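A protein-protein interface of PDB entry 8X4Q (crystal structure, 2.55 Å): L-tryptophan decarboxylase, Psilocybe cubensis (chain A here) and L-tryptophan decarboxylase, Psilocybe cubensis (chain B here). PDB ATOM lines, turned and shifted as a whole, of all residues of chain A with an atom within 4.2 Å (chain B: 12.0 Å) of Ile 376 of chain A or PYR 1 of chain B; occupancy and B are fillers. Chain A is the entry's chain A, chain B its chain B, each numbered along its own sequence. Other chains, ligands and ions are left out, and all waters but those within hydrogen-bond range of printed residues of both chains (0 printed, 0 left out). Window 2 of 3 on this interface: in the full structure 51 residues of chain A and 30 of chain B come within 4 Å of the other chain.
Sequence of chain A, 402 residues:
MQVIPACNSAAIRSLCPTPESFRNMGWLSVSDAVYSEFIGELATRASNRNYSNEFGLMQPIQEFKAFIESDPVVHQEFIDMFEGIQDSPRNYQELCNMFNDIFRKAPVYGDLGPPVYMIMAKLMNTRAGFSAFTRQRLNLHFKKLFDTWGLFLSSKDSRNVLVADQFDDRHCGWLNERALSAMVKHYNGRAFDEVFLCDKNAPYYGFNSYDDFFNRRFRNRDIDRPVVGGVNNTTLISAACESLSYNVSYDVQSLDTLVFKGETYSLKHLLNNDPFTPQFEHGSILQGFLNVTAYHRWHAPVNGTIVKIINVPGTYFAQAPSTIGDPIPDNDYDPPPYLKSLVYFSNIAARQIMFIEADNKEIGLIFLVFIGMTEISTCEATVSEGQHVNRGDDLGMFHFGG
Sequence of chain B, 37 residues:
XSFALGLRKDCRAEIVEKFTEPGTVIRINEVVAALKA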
ATOM      1  N   PRO A 114       8.859   0.068  21.670  1.00  0.00           N
ATOM      2  CA  PRO A 114       9.270   1.151  22.572  1.00  0.00           C
ATOM      3  C   PRO A 114       8.150   1.533  23.533  1.00  0.00           C
ATOM      4  O   PRO A 114       6.978   1.200  23.305  1.00  0.00           O
ATOM      5  CB  PRO A 114       9.607   2.285  21.594  1.00  0.00           C
ATOM      6  CG  PRO A 114       8.752   2.011  20.424  1.00  0.00           C
ATOM      7  CD  PRO A 114       8.768   0.526  20.275  1.00  0.00           C
ATOM      8  N   PHE A 214      21.672   4.634  20.707  1.00  0.00           N
ATOM      9  CA  PHE A 214      20.695   4.301  19.673  1.00  0.00           C
ATOM     10  C   PHE A 214      21.263   4.534  18.282  1.00  0.00           C
ATOM     11  O   PHE A 214      20.941   3.785  17.346  1.00  0.00           O
ATOM     12  CB  PHE A 214      19.431   5.133  19.889  1.00  0.00           C
ATOM     13  CG  PHE A 214      18.322   4.878  18.897  1.00  0.00           C
ATOM     14  CD1 PHE A 214      17.418   3.847  19.098  1.00  0.00           C
ATOM     15  CD2 PHE A 214      18.169   5.686  17.784  1.00  0.00           C
ATOM     16  CE1 PHE A 214      16.384   3.623  18.202  1.00  0.00           C
ATOM     17  CE2 PHE A 214      17.140   5.473  16.876  1.00  0.00           C
ATOM     18  CZ  PHE A 214      16.238   4.438  17.092  1.00  0.00           C
ATOM     19  N   PHE A 289      11.976  -3.235   7.691  1.00  0.00           N
ATOM     20  CA  PHE A 289      11.600  -2.901   9.062  1.00  0.00           C
ATOM     21  C   PHE A 289      12.841  -2.953   9.941  1.00  0.00           C
ATOM     22  O   PHE A 289      13.659  -3.874   9.827  1.00  0.00           O
ATOM     23  CB  PHE A 289      10.517  -3.865   9.553  1.00  0.00           C
ATOM     24  CG  PHE A 289      10.226  -3.793  11.019  1.00  0.00           C
ATOM     25  CD1 PHE A 289       9.877  -2.590  11.627  1.00  0.00           C
ATOM     26  CD2 PHE A 289      10.207  -4.951  11.785  1.00  0.00           C
ATOM     27  CE1 PHE A 289       9.568  -2.542  12.996  1.00  0.00           C
ATOM     28  CE2 PHE A 289       9.897  -4.908  13.142  1.00  0.00           C
ATOM     29  CZ  PHE A 289       9.584  -3.713  13.748  1.00  0.00           C
ATOM     30  N   LEU A 290      13.005  -1.939  10.777  1.00  0.00           N
ATOM     31  CA  LEU A 290      14.154  -1.841  11.671  1.00  0.00           C
ATOM     32  C   LEU A 290      13.676  -2.186  13.077  1.00  0.00           C
ATOM     33  O   LEU A 290      12.840  -1.470  13.652  1.00  0.00           O
ATOM     34  CB  LEU A 290      14.793  -0.449  11.627  1.00  0.00           C
ATOM     35  CG  LEU A 290      15.557   0.051  10.388  1.00  0.00           C
ATOM     36  CD1 LEU A 290      14.659   0.507   9.254  1.00  0.00           C
ATOM     37  CD2 LEU A 290      16.481   1.179  10.775  1.00  0.00           C
ATOM     38  N   ILE A 371      10.542   6.278   7.193  1.00  0.00           N
ATOM     39  CA  ILE A 371       9.184   6.230   7.737  1.00  0.00           C
ATOM     40  C   ILE A 371       9.264   6.049   9.244  1.00  0.00           C
ATOM     41  O   ILE A 371       9.879   5.087   9.729  1.00  0.00           O
ATOM     42  CB  ILE A 371       8.379   5.082   7.109  1.00  0.00           C
ATOM     43  CG1 ILE A 371       8.448   5.172   5.571  1.00  0.00           C
ATOM     44  CG2 ILE A 371       6.941   5.028   7.671  1.00  0.00           C
ATOM     45  CD1 ILE A 371       8.645   3.854   4.873  1.00  0.00           C
ATOM     46  N   GLY A 372       8.630   6.958   9.987  1.00  0.00           N
ATOM     47  CA  GLY A 372       8.587   6.827  11.429  1.00  0.00           C
ATOM     48  C   GLY A 372       7.564   5.805  11.895  1.00  0.00           C
ATOM     49  O   GLY A 372       6.664   5.397  11.162  1.00  0.00           O
ATOM     50  N   MET A 373       7.748   5.376  13.145  1.00  0.00           N
ATOM     51  CA  MET A 373       6.817   4.500  13.861  1.00  0.00           C
ATOM     52  C   MET A 373       6.739   4.966  15.310  1.00  0.00           C
ATOM     53  O   MET A 373       7.743   4.914  16.022  1.00  0.00           O
ATOM     54  CB  MET A 373       7.228   3.020  13.785  1.00  0.00           C
ATOM     55  CG  MET A 373       7.456   2.514  12.362  1.00  0.00           C
ATOM     56  SD  MET A 373       8.015   0.803  12.231  1.00  0.00           S
ATOM     57  CE  MET A 373       6.883   0.001  13.343  1.00  0.00           C
ATOM     58  N   THR A 374       5.544   5.415  15.732  1.00  0.00           N
ATOM     59  CA  THR A 374       5.257   5.924  17.073  1.00  0.00           C
ATOM     60  C   THR A 374       6.319   6.912  17.542  1.00  0.00           C
ATOM     61  O   THR A 374       6.571   7.910  16.860  1.00  0.00           O
ATOM     62  CB  THR A 374       5.068   4.771  18.072  1.00  0.00           C
ATOM     63  OG1 THR A 374       6.287   4.030  18.253  1.00  0.00           O
ATOM     64  CG2 THR A 374       3.975   3.844  17.598  1.00  0.00           C
ATOM     65  N   GLU A 375       6.951   6.667  18.692  1.00  0.00           N
ATOM     66  CA  GLU A 375       7.874   7.658  19.234  1.00  0.00           C
ATOM     67  C   GLU A 375       9.209   7.669  18.521  1.00  0.00           C
ATOM     68  O   GLU A 375      10.002   8.579  18.748  1.00  0.00           O
ATOM     69  CB  GLU A 375       8.125   7.413  20.720  1.00  0.00           C
ATOM     70  CG  GLU A 375       8.774   6.085  20.932  1.00  0.00           C
ATOM     71  CD  GLU A 375       7.821   5.142  21.568  1.00  0.00           C
ATOM     72  OE1 GLU A 375       6.847   4.776  20.872  1.00  0.00           O
ATOM     73  OE2 GLU A 375       8.034   4.749  22.729  1.00  0.00           O
ATOM     74  N   ILE A 376       9.498   6.694  17.676  1.00  0.00           N
ATOM     75  CA  ILE A 376      10.706   6.782  16.860  1.00  0.00           C
ATOM     76  C   ILE A 376      10.326   7.315  15.489  1.00  0.00           C
ATOM     77  O   ILE A 376      10.253   6.558  14.517  1.00  0.00           O
ATOM     78  CB  ILE A 376      11.458   5.433  16.780  1.00  0.00           C
ATOM     79  CG1 ILE A 376      11.586   4.797  18.171  1.00  0.00           C
ATOM     80  CG2 ILE A 376      12.864   5.609  16.182  1.00  0.00           C
ATOM     81  CD1 ILE A 376      11.665   3.306  18.170  1.00  0.00           C
ATOM     82  N   SER A 377      10.093   8.633  15.397  1.00  0.00           N
ATOM     83  CA  SER A 377       9.618   9.217  14.147  1.00  0.00           C
ATOM     84  C   SER A 377      10.402  10.427  13.659  1.00  0.00           C
ATOM     85  O   SER A 377      10.007  11.025  12.649  1.00  0.00           O
ATOM     86  CB  SER A 377       8.145   9.576  14.267  1.00  0.00           C
ATOM     87  OG  SER A 377       7.390   8.384  14.355  1.00  0.00           O
ATOM     88  N   THR A 378      11.506  10.793  14.314  1.00  0.00           N
ATOM     89  CA  THR A 378      12.353  11.886  13.837  1.00  0.00           C
ATOM     90  C   THR A 378      13.287  11.369  12.740  1.00  0.00           C
ATOM     91  O   THR A 378      14.033  10.397  12.950  1.00  0.00           O
ATOM     92  CB  THR A 378      13.190  12.480  14.979  1.00  0.00           C
ATOM     93  OG1 THR A 378      12.349  13.211  15.878  1.00  0.00           O
ATOM     94  CG2 THR A 378      14.177  13.484  14.410  1.00  0.00           C
ATOM     95  N   PHE A 398      17.649   7.796  12.278  1.00  0.00           N
ATOM     96  CA  PHE A 398      16.410   7.900  13.029  1.00  0.00           C
ATOM     97  C   PHE A 398      16.733   8.382  14.439  1.00  0.00           C
ATOM     98  O   PHE A 398      17.822   8.136  14.965  1.00  0.00           O
ATOM     99  CB  PHE A 398      15.700   6.548  13.113  1.00  0.00           C
ATOM    100  CG  PHE A 398      15.009   6.125  11.851  1.00  0.00           C
ATOM    101  CD1 PHE A 398      13.914   6.818  11.358  1.00  0.00           C
ATOM    102  CD2 PHE A 398      15.492   5.040  11.128  1.00  0.00           C
ATOM    103  CE1 PHE A 398      13.281   6.415  10.196  1.00  0.00           C
ATOM    104  CE2 PHE A 398      14.869   4.642   9.947  1.00  0.00           C
ATOM    105  CZ  PHE A 398      13.762   5.326   9.486  1.00  0.00           C
ATOM    106  N   HIS A 399      15.771   9.069  15.054  1.00  0.00           N
ATOM    107  CA  HIS A 399      15.836   9.401  16.471  1.00  0.00           C
ATOM    108  C   HIS A 399      14.482   9.138  17.115  1.00  0.00           C
ATOM    109  O   HIS A 399      13.435   9.255  16.468  1.00  0.00           O
ATOM    110  CB  HIS A 399      16.159  10.877  16.709  1.00  0.00           C
ATOM    111  CG  HIS A 399      17.511  11.301  16.244  1.00  0.00           C
ATOM    112  ND1 HIS A 399      18.655  11.070  16.975  1.00  0.00           N
ATOM    113  CD2 HIS A 399      17.899  11.970  15.129  1.00  0.00           C
ATOM    114  CE1 HIS A 399      19.692  11.570  16.323  1.00  0.00           C
ATOM    115  NE2 HIS A 399      19.260  12.126  15.203  1.00  0.00           N
ATOM    116  N   PHE A 400      14.503   8.817  18.403  1.00  0.00           N
ATOM    117  CA  PHE A 400      13.323   9.047  19.217  1.00  0.00           C
ATOM    118  C   PHE A 400      12.940  10.516  19.107  1.00  0.00           C
ATOM    119  O   PHE A 400      13.773  11.402  19.313  1.00  0.00           O
ATOM    120  CB  PHE A 400      13.600   8.678  20.667  1.00  0.00           C
ATOM    121  CG  PHE A 400      13.426   7.216  20.977  1.00  0.00           C
ATOM    122  CD1 PHE A 400      14.349   6.271  20.523  1.00  0.00           C
ATOM    123  CD2 PHE A 400      12.345   6.782  21.754  1.00  0.00           C
ATOM    124  CE1 PHE A 400      14.188   4.915  20.815  1.00  0.00           C
ATOM    125  CE2 PHE A 400      12.176   5.430  22.066  1.00  0.00           C
ATOM    126  CZ  PHE A 400      13.104   4.492  21.598  1.00  0.00           C
ATOM    127  C   PYR B   1      11.734   1.559  10.675  1.00  0.00           C
ATOM    128  O   PYR B   1      11.393   0.209  10.815  1.00  0.00           O
ATOM    129  CA  PYR B   1      11.652   2.220  12.036  1.00  0.00           C
ATOM    130  O3  PYR B   1      11.996   1.586  12.969  1.00  0.00           O
ATOM    131  CB  PYR B   1      11.138   3.658  12.203  1.00  0.00           C
ATOM    132  N   SER B   2      11.048   2.186   9.591  1.00  0.00           N
ATOM    133  CA  SER B   2      10.903   1.573   8.290  1.00  0.00           C
ATOM    134  C   SER B   2      11.537   2.480   7.260  1.00  0.00           C
ATOM    135  O   SER B   2      11.533   3.706   7.427  1.00  0.00           O
ATOM    136  CB  SER B   2       9.420   1.334   7.966  1.00  0.00           C
ATOM    137  OG  SER B   2       9.249   0.374   6.938  1.00  0.00           O
ATOM    138  N   PHE B   3      12.085   1.886   6.197  1.00  0.00           N
ATOM    139  CA  PHE B   3      12.542   2.645   5.040  1.00  0.00           C
ATOM    140  C   PHE B   3      12.014   2.016   3.753  1.00  0.00           C
ATOM    141  O   PHE B   3      11.724   0.812   3.696  1.00  0.00           O
ATOM    142  CB  PHE B   3      14.070   2.744   4.994  1.00  0.00           C
ATOM    143  CG  PHE B   3      14.721   1.605   4.296  1.00  0.00           C
ATOM    144  CD1 PHE B   3      14.921   0.409   4.958  1.00  0.00           C
ATOM    145  CD2 PHE B   3      15.144   1.724   2.984  1.00  0.00           C
ATOM    146  CE1 PHE B   3      15.519  -0.653   4.325  1.00  0.00           C
ATOM    147  CE2 PHE B   3      15.752   0.655   2.336  1.00  0.00           C
ATOM    148  CZ  PHE B   3      15.941  -0.533   3.007  1.00  0.00           C
ATOM    149  N   ALA B   4      11.872   2.851   2.720  1.00  0.00           N
ATOM    150  CA  ALA B   4      11.477   2.382   1.404  1.00  0.00           C
ATOM    151  C   ALA B   4      12.420   2.919   0.337  1.00  0.00           C
ATOM    152  O   ALA B   4      12.768   4.102   0.340  1.00  0.00           O
ATOM    153  CB  ALA B   4      10.045   2.786   1.073  1.00  0.00           C
ATOM    154  N   LEU B   5      12.842   2.031  -0.564  1.00  0.00           N
ATOM    155  CA  LEU B   5      13.567   2.391  -1.774  1.00  0.00           C
ATOM    156  C   LEU B   5      12.601   2.310  -2.952  1.00  0.00           C
ATOM    157  O   LEU B   5      11.855   1.329  -3.076  1.00  0.00           O
ATOM    158  CB  LEU B   5      14.754   1.455  -1.979  1.00  0.00           C
ATOM    159  CG  LEU B   5      15.488   1.595  -3.304  1.00  0.00           C
ATOM    160  CD1 LEU B   5      16.453   2.771  -3.226  1.00  0.00           C
ATOM    161  CD2 LEU B   5      16.227   0.312  -3.623  1.00  0.00           C
ATOM    162  N   THR B  24      13.359 -11.601   5.489  1.00  0.00           N
ATOM    163  CA  THR B  24      14.735 -11.826   5.075  1.00  0.00           C
ATOM    164  C   THR B  24      15.634 -10.731   5.645  1.00  0.00           C
ATOM    165  O   THR B  24      15.280  -9.545   5.646  1.00  0.00           O
ATOM    166  CB  THR B  24      14.814 -11.842   3.552  1.00  0.00           C
ATOM    167  OG1 THR B  24      13.738 -12.630   3.041  1.00  0.00           O
ATOM    168  CG2 THR B  24      16.148 -12.397   3.051  1.00  0.00           C
ATOM    169  N   ILE B  26      18.231  -7.944   5.953  1.00  0.00           N
ATOM    170  CA  ILE B  26      18.841  -6.957   5.068  1.00  0.00           C
ATOM    171  C   ILE B  26      20.037  -6.362   5.796  1.00  0.00           C
ATOM    172  O   ILE B  26      19.889  -5.589   6.752  1.00  0.00           O
ATOM    173  CB  ILE B  26      17.860  -5.862   4.638  1.00  0.00           C
ATOM    174  CG1 ILE B  26      16.765  -6.415   3.736  1.00  0.00           C
ATOM    175  CG2 ILE B  26      18.594  -4.839   3.866  1.00  0.00           C
ATOM    176  CD1 ILE B  26      15.706  -5.350   3.386  1.00  0.00           C
ATOM    177  N   ILE B  28      22.826  -3.801   6.056  1.00  0.00           N
ATOM    178  CA  ILE B  28      23.055  -2.478   5.505  1.00  0.00           C
ATOM    179  C   ILE B  28      24.299  -2.520   4.622  1.00  0.00           C
ATOM    180  O   ILE B  28      25.282  -3.210   4.927  1.00  0.00           O
ATOM    181  CB  ILE B  28      23.144  -1.450   6.649  1.00  0.00           C
ATOM    182  CG1 ILE B  28      22.881  -0.029   6.127  1.00  0.00           C
ATOM    183  CG2 ILE B  28      24.453  -1.609   7.438  1.00  0.00           C
ATOM    184  CD1 ILE B  28      23.079   1.045   7.152  1.00  0.00           C
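PYR 1 of chain B touches Phe 289 of chain A. CD1 of Leu 290 of chain A touches N of Ser 2 of chain B, 3.996 Å away. PYR 1 of chain B touches Ile 371 of chain A. Ile 371 of chain A touches Phe 3 of chain B. PYR 1 of chain B touches Ile 376 of chain A. O of Ser 2 of chain B touches CZ of Phe 398 of chain A (3.4 Å).
Printed residues of chain B that touch a printed residue of chain A: PYR 1, Ser 2 and Phe 3. Hydrophobic or aromatic side chains of chain A that line the printed part of chain B: Phe 289, Leu 290, Ile 371, Met 373 and Phe 398. Along chain A the printed residues that touch a printed residue of chain B span positions 289 to 398. Among the printed residues, 9 pairs touch across the chains.
N of Leu 290 of chain A sits at hydrogen-bond distance from O of PYR 1 of chain B (2.7 Å). N of Ile 371 of chain A is in hydrogen-bond range of O of Ser 2 of chain B, 2.8 Å away. O of PYR 1 of chain B lies close to the side-chain sulfur of Met 373 of chain A (3.7 Å).
No residue of chain B comes within 4 Å of Pro 114 of chain A. Phe 289 of chain A touches just one residue of chain B: PYR 1 (3.3 Å). Printed residues of chain B within 4 Å of Leu 290 of chain A: PYR 1 (2.7 Å) and Ser 2 (3.996 Å). Of the printed residues of chain B, Ile 371 of chain A touches PYR 1 (3.1 Å), Ser 2 (2.8 Å) and Phe 3 (3.998 Å). No residue of chain B comes within 4 Å of Gly 372 of chain A. Of chain B, only PYR 1 comes within 4 Å of Met 373 of chain A. No residue of chain B comes within 4 Å of Thr 374 of chain A. No residue of chain B comes within 4 Å of Glu 375 of chain A. No residue of chain B comes within 4 Å of Thr 378 of chain A. His 399 of chain A touches none of the printed residues of chain B. No residue of chain B comes within 4 Å of Phe 400 of chain A. Of chain A, only Phe 289 (3.3 Å), Leu 290 (2.7 Å), Ile 371 (3.1 Å), Met 373 (3.7 Å) and Ile 376 (3.8 Å) come within 4 Å of PYR 1 of chain B. Printed residues of chain A within 4 Å of Ser 2 of chain B: Leu 290 (3.996 Å), Ile 371 (2.8 Å) and Phe 398 (3.4 Å). Of the printed residues of chain A, Phe 3 of chain B touches Ile 371. Leu 5 of chain B touches none of the printed residues of chain A. The nearest residue of chain B that does not touch Ile 376 of chain A is Ser 2 of chain B (6.6 Å).
The backbone NH (N) of Met 373 of chain A is in hydrogen-bond range of the side-chain hydroxyl (OG) of Ser 377 of chain A.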
